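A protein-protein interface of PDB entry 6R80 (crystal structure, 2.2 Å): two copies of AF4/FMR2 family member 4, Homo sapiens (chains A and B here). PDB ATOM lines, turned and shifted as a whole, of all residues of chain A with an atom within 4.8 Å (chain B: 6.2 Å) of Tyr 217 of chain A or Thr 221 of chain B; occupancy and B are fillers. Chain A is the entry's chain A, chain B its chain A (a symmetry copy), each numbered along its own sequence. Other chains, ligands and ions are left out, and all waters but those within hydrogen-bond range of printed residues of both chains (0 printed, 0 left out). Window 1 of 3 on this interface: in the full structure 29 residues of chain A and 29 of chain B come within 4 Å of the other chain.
Hydrophobic or aromatic side chains of chain B within 4 Å of the printed part of chain A: Phe 135, Ala 142, Tyr 217, Val 218 and Leu 225.
Among the printed residues, no Asp or Glu carboxylate lies within 4 Å of a Lys or Arg side-chain nitrogen of the other chain.
The side-chain hydroxyl (OG) of Ser 222 of chain B is in hydrogen-bond range of the backbone carbonyl oxygen (O) of Gln 219 of chain B (2.6 Å).
The side-chain hydroxyl (OG1) of Thr 221 of chain B lies within hydrogen-bond range of the backbone carbonyl oxygen (O) of Val 218 of chain B, at 3.2 Å.
The side-chain hydroxyl of Thr 221 of chain B sits at hydrogen-bond distance from the backbone carbonyl oxygen of Tyr 217 of chain B, at 2.7 Å.
O of Gln 219 of chain A sits at hydrogen-bond distance from OG of Ser 222 of chain A, 2.6 Å away.
The side-chain hydroxyl of Thr 221 of chain A is in hydrogen-bond range of the backbone carbonyl oxygen of Tyr 217 of chain A.
The side-chain hydroxyl (OG1) of Thr 221 of chain A sits at hydrogen-bond distance from the backbone carbonyl oxygen (O) of Val 218 of chain A, at 3.2 Å.
CD1 of Leu 225 of chain B touches O of Ala 142 of chain A (3.7 Å).
Ser 146 of chain A touches Val 218 of chain B (O to CG1, 3.8 Å).
Ser 146 of chain A touches Ser 222 of chain B.
Ser 146 of chain A touches Leu 225 of chain B (CB to CD1, 3.9 Å).
Tyr 217 of chain A touches Ser 222 of chain B.
Leu 225 of chain B touches Tyr 217 of chain A.
Tyr 217 of chain B touches Ser 222 of chain A (OH to N, 3.6 Å).
Phe 135 of chain B touches Leu 225 of chain A.
Leu 225 of chain A touches Ala 142 of chain B.
OH of Tyr 217 of chain B touches CD1 of Leu 225 of chain A, 3.5 Å away.
Tyr 217 of chain A touches Val 218 of chain B, and with the chains exchanged Val 218 of chain A touches Tyr 217 of chain B.
Tyr 217 of chain A touches Thr 221 of chain B, and with the chains exchanged Thr 221 of chain A touches Tyr 217 of chain B.
Tyr 217 of chain A touches Ser 222 of chain B, and with the chains exchanged Ser 222 of chain A touches Tyr 217 of chain B.
Tyr 217 of chain A touches Leu 225 of chain B, and with the chains exchanged Leu 225 of chain A touches Tyr 217 of chain B.
Positions printed for both chains: 142, 216, 217, 218, 219, 220, 221, 222 and 225.
Of the 14 pairs that touch across the chains among the printed residues, 10 have their exchanged pair printed and touching as well.
Tyr 217 of chain A touches four residues of chain B.
Thr 221 of chain B touches just one residue of chain A: Tyr 217.
Of the printed residues of chain B, Ser 222 of chain A touches Tyr 217 (3.6 Å).
Printed residues of chain B within 4 Å of Ala 142 of chain A: Leu 225 (3.7 Å).
Printed residues of chain B within 4 Å of Thr 221 of chain A: Tyr 217 (2.6 Å).
Of the printed residues of chain A, Tyr 217 of chain B touches Val 218, Thr 221, Ser 222 and Leu 225.
Of the printed residues of chain A, Ser 222 of chain B touches Ser 146 (3.97 Å) and Tyr 217 (3.6 Å).
Val 220 of chain B touches none of the printed residues of chain A.
The nearest residue of chain A that does not touch Thr 221 of chain B is Thr 221 of chain A (4.1 Å).
The backbone carbonyl oxygen (O) of Val 218 of chain A lies within hydrogen-bond range of the side-chain hydroxyl (OH) of Tyr 217 of chain B.
The side-chain hydroxyl of Tyr 217 of chain A sits at hydrogen-bond distance from the backbone carbonyl oxygen of Val 218 of chain B (3.5 Å).
The side-chain hydroxyl of Tyr 217 of chain A lies within hydrogen-bond range of the side-chain hydroxyl of Thr 221 of chain B.
The side-chain hydroxyl (OH) of Tyr 217 of chain B is in hydrogen-bond range of the side-chain hydroxyl (OG1) of Thr 221 of chain A, at 2.6 Å.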
ATOM      1  N   ALA A 142      -3.469  16.349  20.300  1.00  0.00           N
ATOM      2  CA  ALA A 142      -3.626  17.729  19.852  1.00  0.00           C
ATOM      3  C   ALA A 142      -3.389  17.867  18.354  1.00  0.00           C
ATOM      4  O   ALA A 142      -4.089  18.629  17.678  1.00  0.00           O
ATOM      5  CB  ALA A 142      -2.680  18.642  20.631  1.00  0.00           C
ATOM      6  N   TYR A 145      -6.383  16.218  16.374  1.00  0.00           N
ATOM      7  CA  TYR A 145      -7.553  17.072  16.534  1.00  0.00           C
ATOM      8  C   TYR A 145      -7.421  18.356  15.732  1.00  0.00           C
ATOM      9  O   TYR A 145      -8.412  18.856  15.190  1.00  0.00           O
ATOM     10  CB  TYR A 145      -7.771  17.404  18.014  1.00  0.00           C
ATOM     11  CG  TYR A 145      -8.150  16.225  18.888  1.00  0.00           C
ATOM     12  CD1 TYR A 145      -8.659  15.056  18.338  1.00  0.00           C
ATOM     13  CD2 TYR A 145      -8.007  16.289  20.269  1.00  0.00           C
ATOM     14  CE1 TYR A 145      -9.010  13.982  19.139  1.00  0.00           C
ATOM     15  CE2 TYR A 145      -8.352  15.220  21.076  1.00  0.00           C
ATOM     16  CZ  TYR A 145      -8.854  14.071  20.507  1.00  0.00           C
ATOM     17  OH  TYR A 145      -9.200  13.005  21.307  1.00  0.00           O
ATOM     18  N   SER A 146      -6.205  18.896  15.637  1.00  0.00           N
ATOM     19  CA  SER A 146      -5.984  20.130  14.888  1.00  0.00           C
ATOM     20  C   SER A 146      -6.379  19.969  13.426  1.00  0.00           C
ATOM     21  O   SER A 146      -7.051  20.835  12.853  1.00  0.00           O
ATOM     22  CB  SER A 146      -4.519  20.551  15.002  1.00  0.00           C
ATOM     23  OG  SER A 146      -4.012  20.976  13.750  1.00  0.00           O
ATOM     24  N   LEU A 149     -10.313  19.322  13.232  1.00  0.00           N
ATOM     25  CA  LEU A 149     -11.096  20.516  13.539  1.00  0.00           C
ATOM     26  C   LEU A 149     -11.028  21.528  12.404  1.00  0.00           C
ATOM     27  O   LEU A 149     -12.053  22.077  11.984  1.00  0.00           O
ATOM     28  CB  LEU A 149     -10.613  21.144  14.848  1.00  0.00           C
ATOM     29  CG  LEU A 149     -10.929  20.406  16.150  1.00  0.00           C
ATOM     30  CD1 LEU A 149     -10.258  21.095  17.333  1.00  0.00           C
ATOM     31  CD2 LEU A 149     -12.432  20.297  16.362  1.00  0.00           C
ATOM     32  N   MET A 213     -14.263  17.562  20.874  1.00  0.00           N
ATOM     33  CA  MET A 213     -12.905  17.552  20.344  1.00  0.00           C
ATOM     34  C   MET A 213     -12.324  18.955  20.393  1.00  0.00           C
ATOM     35  O   MET A 213     -11.153  19.143  20.717  1.00  0.00           O
ATOM     36  CB  MET A 213     -12.878  17.021  18.910  1.00  0.00           C
ATOM     37  CG  MET A 213     -11.501  17.078  18.266  1.00  0.00           C
ATOM     38  SD  MET A 213     -11.474  16.533  16.393  1.00  0.00           S
ATOM     39  CE  MET A 213     -12.033  14.673  16.588  1.00  0.00           C
ATOM     40  N   ALA A 214     -13.158  19.943  20.064  1.00  0.00           N
ATOM     41  CA  ALA A 214     -12.732  21.334  20.174  1.00  0.00           C
ATOM     42  C   ALA A 214     -12.443  21.699  21.624  1.00  0.00           C
ATOM     43  O   ALA A 214     -11.433  22.345  21.924  1.00  0.00           O
ATOM     44  CB  ALA A 214     -13.798  22.259  19.586  1.00  0.00           C
ATOM     45  N   ALA A 215     -13.324  21.284  22.540  1.00  0.00           N
ATOM     46  CA  ALA A 215     -13.166  21.637  23.947  1.00  0.00           C
ATOM     47  C   ALA A 215     -11.852  21.111  24.508  1.00  0.00           C
ATOM     48  O   ALA A 215     -11.098  21.847  25.157  1.00  0.00           O
ATOM     49  CB  ALA A 215     -14.350  21.102  24.755  1.00  0.00           C
ATOM     50  N   SER A 216     -11.551  19.836  24.256  1.00  0.00           N
ATOM     51  CA  SER A 216     -10.321  19.255  24.784  1.00  0.00           C
ATOM     52  C   SER A 216      -9.092  19.808  24.071  1.00  0.00           C
ATOM     53  O   SER A 216      -8.039  19.990  24.695  1.00  0.00           O
ATOM     54  CB  SER A 216     -10.364  17.732  24.673  1.00  0.00           C
ATOM     55  OG  SER A 216     -10.399  17.323  23.317  1.00  0.00           O
ATOM     56  N   TYR A 217      -9.198  20.068  22.765  1.00  0.00           N
ATOM     57  CA  TYR A 217      -8.075  20.659  22.043  1.00  0.00           C
ATOM     58  C   TYR A 217      -7.698  22.010  22.635  1.00  0.00           C
ATOM     59  O   TYR A 217      -6.512  22.333  22.760  1.00  0.00           O
ATOM     60  CB  TYR A 217      -8.408  20.803  20.557  1.00  0.00           C
ATOM     61  CG  TYR A 217      -7.327  21.512  19.766  1.00  0.00           C
ATOM     62  CD1 TYR A 217      -6.251  20.810  19.244  1.00  0.00           C
ATOM     63  CD2 TYR A 217      -7.380  22.884  19.550  1.00  0.00           C
ATOM     64  CE1 TYR A 217      -5.257  21.452  18.523  1.00  0.00           C
ATOM     65  CE2 TYR A 217      -6.392  23.536  18.834  1.00  0.00           C
ATOM     66  CZ  TYR A 217      -5.333  22.816  18.322  1.00  0.00           C
ATOM     67  OH  TYR A 217      -4.348  23.459  17.606  1.00  0.00           O
ATOM     68  N   VAL A 218      -8.696  22.817  22.995  1.00  0.00           N
ATOM     69  CA  VAL A 218      -8.421  24.092  23.648  1.00  0.00           C
ATOM     70  C   VAL A 218      -7.743  23.859  24.992  1.00  0.00           C
ATOM     71  O   VAL A 218      -6.806  24.574  25.364  1.00  0.00           O
ATOM     72  CB  VAL A 218      -9.722  24.903  23.792  1.00  0.00           C
ATOM     73  CG1 VAL A 218      -9.523  26.072  24.740  1.00  0.00           C
ATOM     74  CG2 VAL A 218     -10.193  25.390  22.425  1.00  0.00           C
ATOM     75  N   GLN A 219      -8.181  22.833  25.723  1.00  0.00           N
ATOM     76  CA  GLN A 219      -7.628  22.561  27.048  1.00  0.00           C
ATOM     77  C   GLN A 219      -6.156  22.172  26.963  1.00  0.00           C
ATOM     78  O   GLN A 219      -5.326  22.665  27.736  1.00  0.00           O
ATOM     79  CB  GLN A 219      -8.447  21.462  27.731  1.00  0.00           C
ATOM     80  CG  GLN A 219      -8.172  21.302  29.217  1.00  0.00           C
ATOM     81  CD  GLN A 219      -9.406  20.874  29.993  1.00  0.00           C
ATOM     82  OE1 GLN A 219     -10.336  20.293  29.433  1.00  0.00           O
ATOM     83  NE2 GLN A 219      -9.425  21.174  31.287  1.00  0.00           N
ATOM     84  N   VAL A 220      -5.810  21.290  26.021  1.00  0.00           N
ATOM     85  CA  VAL A 220      -4.432  20.819  25.916  1.00  0.00           C
ATOM     86  C   VAL A 220      -3.519  21.935  25.418  1.00  0.00           C
ATOM     87  O   VAL A 220      -2.443  22.175  25.979  1.00  0.00           O
ATOM     88  CB  VAL A 220      -4.354  19.574  25.012  1.00  0.00           C
ATOM     89  CG1 VAL A 220      -2.908  19.272  24.637  1.00  0.00           C
ATOM     90  CG2 VAL A 220      -4.989  18.376  25.707  1.00  0.00           C
ATOM     91  N   THR A 221      -3.934  22.638  24.360  1.00  0.00           N
ATOM     92  CA  THR A 221      -3.112  23.724  23.834  1.00  0.00           C
ATOM     93  C   THR A 221      -3.007  24.884  24.816  1.00  0.00           C
ATOM     94  O   THR A 221      -2.022  25.630  24.784  1.00  0.00           O
ATOM     95  CB  THR A 221      -3.668  24.217  22.498  1.00  0.00           C
ATOM     96  OG1 THR A 221      -5.040  24.595  22.659  1.00  0.00           O
ATOM     97  CG2 THR A 221      -3.563  23.129  21.439  1.00  0.00           C
ATOM     98  N   SER A 222      -4.004  25.054  25.689  1.00  0.00           N
ATOM     99  CA  SER A 222      -3.922  26.092  26.711  1.00  0.00           C
ATOM    100  C   SER A 222      -2.738  25.854  27.641  1.00  0.00           C
ATOM    101  O   SER A 222      -1.977  26.782  27.932  1.00  0.00           O
ATOM    102  CB  SER A 222      -5.217  26.150  27.517  1.00  0.00           C
ATOM    103  OG  SER A 222      -5.226  25.148  28.519  1.00  0.00           O
ATOM    104  N   LEU A 225       0.048  27.411  26.254  1.00  0.00           N
ATOM    105  CA  LEU A 225      -0.047  28.866  26.298  1.00  0.00           C
ATOM    106  C   LEU A 225       0.382  29.395  27.658  1.00  0.00           C
ATOM    107  O   LEU A 225       1.072  30.414  27.746  1.00  0.00           O
ATOM    108  CB  LEU A 225      -1.470  29.314  25.966  1.00  0.00           C
ATOM    109  CG  LEU A 225      -1.985  29.017  24.558  1.00  0.00           C
ATOM    110  CD1 LEU A 225      -3.466  29.357  24.454  1.00  0.00           C
ATOM    111  CD2 LEU A 225      -1.182  29.784  23.515  1.00  0.00           C
ATOM    112  N   PHE B 135       3.404  31.517  15.384  1.00  0.00           N
ATOM    113  CA  PHE B 135       2.574  31.449  16.580  1.00  0.00           C
ATOM    114  C   PHE B 135       2.746  32.695  17.439  1.00  0.00           C
ATOM    115  O   PHE B 135       1.764  33.326  17.840  1.00  0.00           O
ATOM    116  CB  PHE B 135       2.912  30.194  17.385  1.00  0.00           C
ATOM    117  CG  PHE B 135       2.604  30.314  18.852  1.00  0.00           C
ATOM    118  CD1 PHE B 135       1.297  30.460  19.292  1.00  0.00           C
ATOM    119  CD2 PHE B 135       3.620  30.277  19.792  1.00  0.00           C
ATOM    120  CE1 PHE B 135       1.012  30.574  20.641  1.00  0.00           C
ATOM    121  CE2 PHE B 135       3.340  30.387  21.142  1.00  0.00           C
ATOM    122  CZ  PHE B 135       2.036  30.536  21.567  1.00  0.00           C
ATOM    123  N   ALA B 142      -4.400  34.261  21.004  1.00  0.00           N
ATOM    124  CA  ALA B 142      -4.615  32.864  21.370  1.00  0.00           C
ATOM    125  C   ALA B 142      -5.013  32.720  22.833  1.00  0.00           C
ATOM    126  O   ALA B 142      -5.866  31.890  23.169  1.00  0.00           O
ATOM    127  CB  ALA B 142      -3.358  32.047  21.073  1.00  0.00           C
ATOM    128  N   SER B 216      -9.778  30.190  14.101  1.00  0.00           N
ATOM    129  CA  SER B 216      -8.492  30.880  14.124  1.00  0.00           C
ATOM    130  C   SER B 216      -7.631  30.418  15.294  1.00  0.00           C
ATOM    131  O   SER B 216      -6.403  30.335  15.170  1.00  0.00           O
ATOM    132  CB  SER B 216      -8.703  32.392  14.180  1.00  0.00           C
ATOM    133  OG  SER B 216      -9.334  32.772  15.390  1.00  0.00           O
ATOM    134  N   TYR B 217      -8.251  30.126  16.442  1.00  0.00           N
ATOM    135  CA  TYR B 217      -7.486  29.617  17.577  1.00  0.00           C
ATOM    136  C   TYR B 217      -6.786  28.313  17.221  1.00  0.00           C
ATOM    137  O   TYR B 217      -5.634  28.092  17.608  1.00  0.00           O
ATOM    138  CB  TYR B 217      -8.395  29.419  18.791  1.00  0.00           C
ATOM    139  CG  TYR B 217      -7.688  28.788  19.973  1.00  0.00           C
ATOM    140  CD1 TYR B 217      -6.990  29.567  20.884  1.00  0.00           C
ATOM    141  CD2 TYR B 217      -7.713  27.412  20.172  1.00  0.00           C
ATOM    142  CE1 TYR B 217      -6.338  28.996  21.964  1.00  0.00           C
ATOM    143  CE2 TYR B 217      -7.063  26.831  21.247  1.00  0.00           C
ATOM    144  CZ  TYR B 217      -6.377  27.627  22.141  1.00  0.00           C
ATOM    145  OH  TYR B 217      -5.731  27.055  23.214  1.00  0.00           O
ATOM    146  N   VAL B 218      -7.473  27.433  16.492  1.00  0.00           N
ATOM    147  CA  VAL B 218      -6.846  26.197  16.036  1.00  0.00           C
ATOM    148  C   VAL B 218      -5.691  26.510  15.094  1.00  0.00           C
ATOM    149  O   VAL B 218      -4.629  25.881  15.159  1.00  0.00           O
ATOM    150  CB  VAL B 218      -7.897  25.284  15.378  1.00  0.00           C
ATOM    151  CG1 VAL B 218      -7.225  24.152  14.620  1.00  0.00           C
ATOM    152  CG2 VAL B 218      -8.853  24.735  16.432  1.00  0.00           C
ATOM    153  N   GLN B 219      -5.868  27.508  14.228  1.00  0.00           N
ATOM    154  CA  GLN B 219      -4.838  27.849  13.250  1.00  0.00           C
ATOM    155  C   GLN B 219      -3.573  28.357  13.934  1.00  0.00           C
ATOM    156  O   GLN B 219      -2.459  27.948  13.586  1.00  0.00           O
ATOM    157  CB  GLN B 219      -5.385  28.889  12.267  1.00  0.00           C
ATOM    158  CG  GLN B 219      -4.530  29.098  11.029  1.00  0.00           C
ATOM    159  CD  GLN B 219      -5.359  29.437   9.801  1.00  0.00           C
ATOM    160  OE1 GLN B 219      -6.482  29.929   9.912  1.00  0.00           O
ATOM    161  NE2 GLN B 219      -4.811  29.160   8.623  1.00  0.00           N
ATOM    162  N   VAL B 220      -3.725  29.247  14.917  1.00  0.00           N
ATOM    163  CA  VAL B 220      -2.560  29.829  15.580  1.00  0.00           C
ATOM    164  C   VAL B 220      -1.849  28.784  16.433  1.00  0.00           C
ATOM    165  O   VAL B 220      -0.622  28.643  16.376  1.00  0.00           O
ATOM    166  CB  VAL B 220      -2.970  31.059  16.411  1.00  0.00           C
ATOM    167  CG1 VAL B 220      -1.843  31.473  17.349  1.00  0.00           C
ATOM    168  CG2 VAL B 220      -3.354  32.213  15.492  1.00  0.00           C
ATOM    169  N   THR B 221      -2.608  28.030  17.234  1.00  0.00           N
ATOM    170  CA  THR B 221      -1.994  27.005  18.074  1.00  0.00           C
ATOM    171  C   THR B 221      -1.393  25.876  17.246  1.00  0.00           C
ATOM    172  O   THR B 221      -0.453  25.214  17.700  1.00  0.00           O
ATOM    173  CB  THR B 221      -3.013  26.444  19.065  1.00  0.00           C
ATOM    174  OG1 THR B 221      -4.156  25.957  18.354  1.00  0.00           O
ATOM    175  CG2 THR B 221      -3.450  27.518  20.052  1.00  0.00           C
ATOM    176  N   SER B 222      -1.918  25.640  16.040  1.00  0.00           N
ATOM    177  CA  SER B 222      -1.331  24.631  15.165  1.00  0.00           C
ATOM    178  C   SER B 222       0.108  24.983  14.809  1.00  0.00           C
ATOM    179  O   SER B 222       0.995  24.127  14.879  1.00  0.00           O
ATOM    180  CB  SER B 222      -2.163  24.481  13.893  1.00  0.00           C
ATOM    181  OG  SER B 222      -1.836  25.497  12.961  1.00  0.00           O
ATOM    182  N   ASN B 223       0.351  26.240  14.424  1.00  0.00           N
ATOM    183  CA  ASN B 223       1.708  26.710  14.144  1.00  0.00           C
ATOM    184  C   ASN B 223       2.686  26.294  15.232  1.00  0.00           C
ATOM    185  O   ASN B 223       3.824  25.909  14.937  1.00  0.00           O
ATOM    186  CB  ASN B 223       1.716  28.233  13.985  1.00  0.00           C
ATOM    187  CG  ASN B 223       1.136  28.686  12.661  1.00  0.00           C
ATOM    188  OD1 ASN B 223       1.311  28.027  11.636  1.00  0.00           O
ATOM    189  ND2 ASN B 223       0.438  29.816  12.676  1.00  0.00           N
ATOM    190  N   PHE B 224       2.272  26.348  16.499  1.00  0.00           N
ATOM    191  CA  PHE B 224       3.177  25.854  17.526  1.00  0.00           C
ATOM    192  C   PHE B 224       3.296  24.339  17.477  1.00  0.00           C
ATOM    193  O   PHE B 224       4.390  23.795  17.667  1.00  0.00           O
ATOM    194  CB  PHE B 224       2.758  26.261  18.932  1.00  0.00           C
ATOM    195  CG  PHE B 224       3.627  25.628  19.969  1.00  0.00           C
ATOM    196  CD1 PHE B 224       4.970  25.963  20.026  1.00  0.00           C
ATOM    197  CD2 PHE B 224       3.153  24.626  20.800  1.00  0.00           C
ATOM    198  CE1 PHE B 224       5.814  25.364  20.930  1.00  0.00           C
ATOM    199  CE2 PHE B 224       3.994  24.024  21.721  1.00  0.00           C
ATOM    200  CZ  PHE B 224       5.326  24.395  21.782  1.00  0.00           C
ATOM    201  N   LEU B 225       2.181  23.636  17.259  1.00  0.00           N
ATOM    202  CA  LEU B 225       2.233  22.180  17.206  1.00  0.00           C
ATOM    203  C   LEU B 225       3.232  21.713  16.158  1.00  0.00           C
ATOM    204  O   LEU B 225       3.978  20.756  16.384  1.00  0.00           O
ATOM    205  CB  LEU B 225       0.843  21.610  16.922  1.00  0.00           C
ATOM    206  CG  LEU B 225      -0.234  21.838  17.982  1.00  0.00           C
ATOM    207  CD1 LEU B 225      -1.590  21.375  17.465  1.00  0.00           C
ATOM    208  CD2 LEU B 225       0.120  21.121  19.278  1.00  0.00           C
ATOM    209  N   TYR B 226       3.273  22.396  15.011  1.00  0.00           N
ATOM    210  CA  TYR B 226       4.255  22.065  13.986  1.00  0.00           C
ATOM    211  C   TYR B 226       5.666  22.411  14.445  1.00  0.00           C
ATOM    212  O   TYR B 226       6.614  21.670  14.164  1.00  0.00           O
ATOM    213  CB  TYR B 226       3.920  22.789  12.679  1.00  0.00           C
ATOM    214  CG  TYR B 226       2.523  22.512  12.165  1.00  0.00           C
ATOM    215  CD1 TYR B 226       2.133  21.225  11.820  1.00  0.00           C
ATOM    216  CD2 TYR B 226       1.598  23.538  12.016  1.00  0.00           C
ATOM    217  CE1 TYR B 226       0.859  20.965  11.353  1.00  0.00           C
ATOM    218  CE2 TYR B 226       0.319  23.287  11.550  1.00  0.00           C
ATOM    219  CZ  TYR B 226      -0.043  21.999  11.219  1.00  0.00           C
ATOM    220  OH  TYR B 226      -1.311  21.737  10.751  1.00  0.00           O
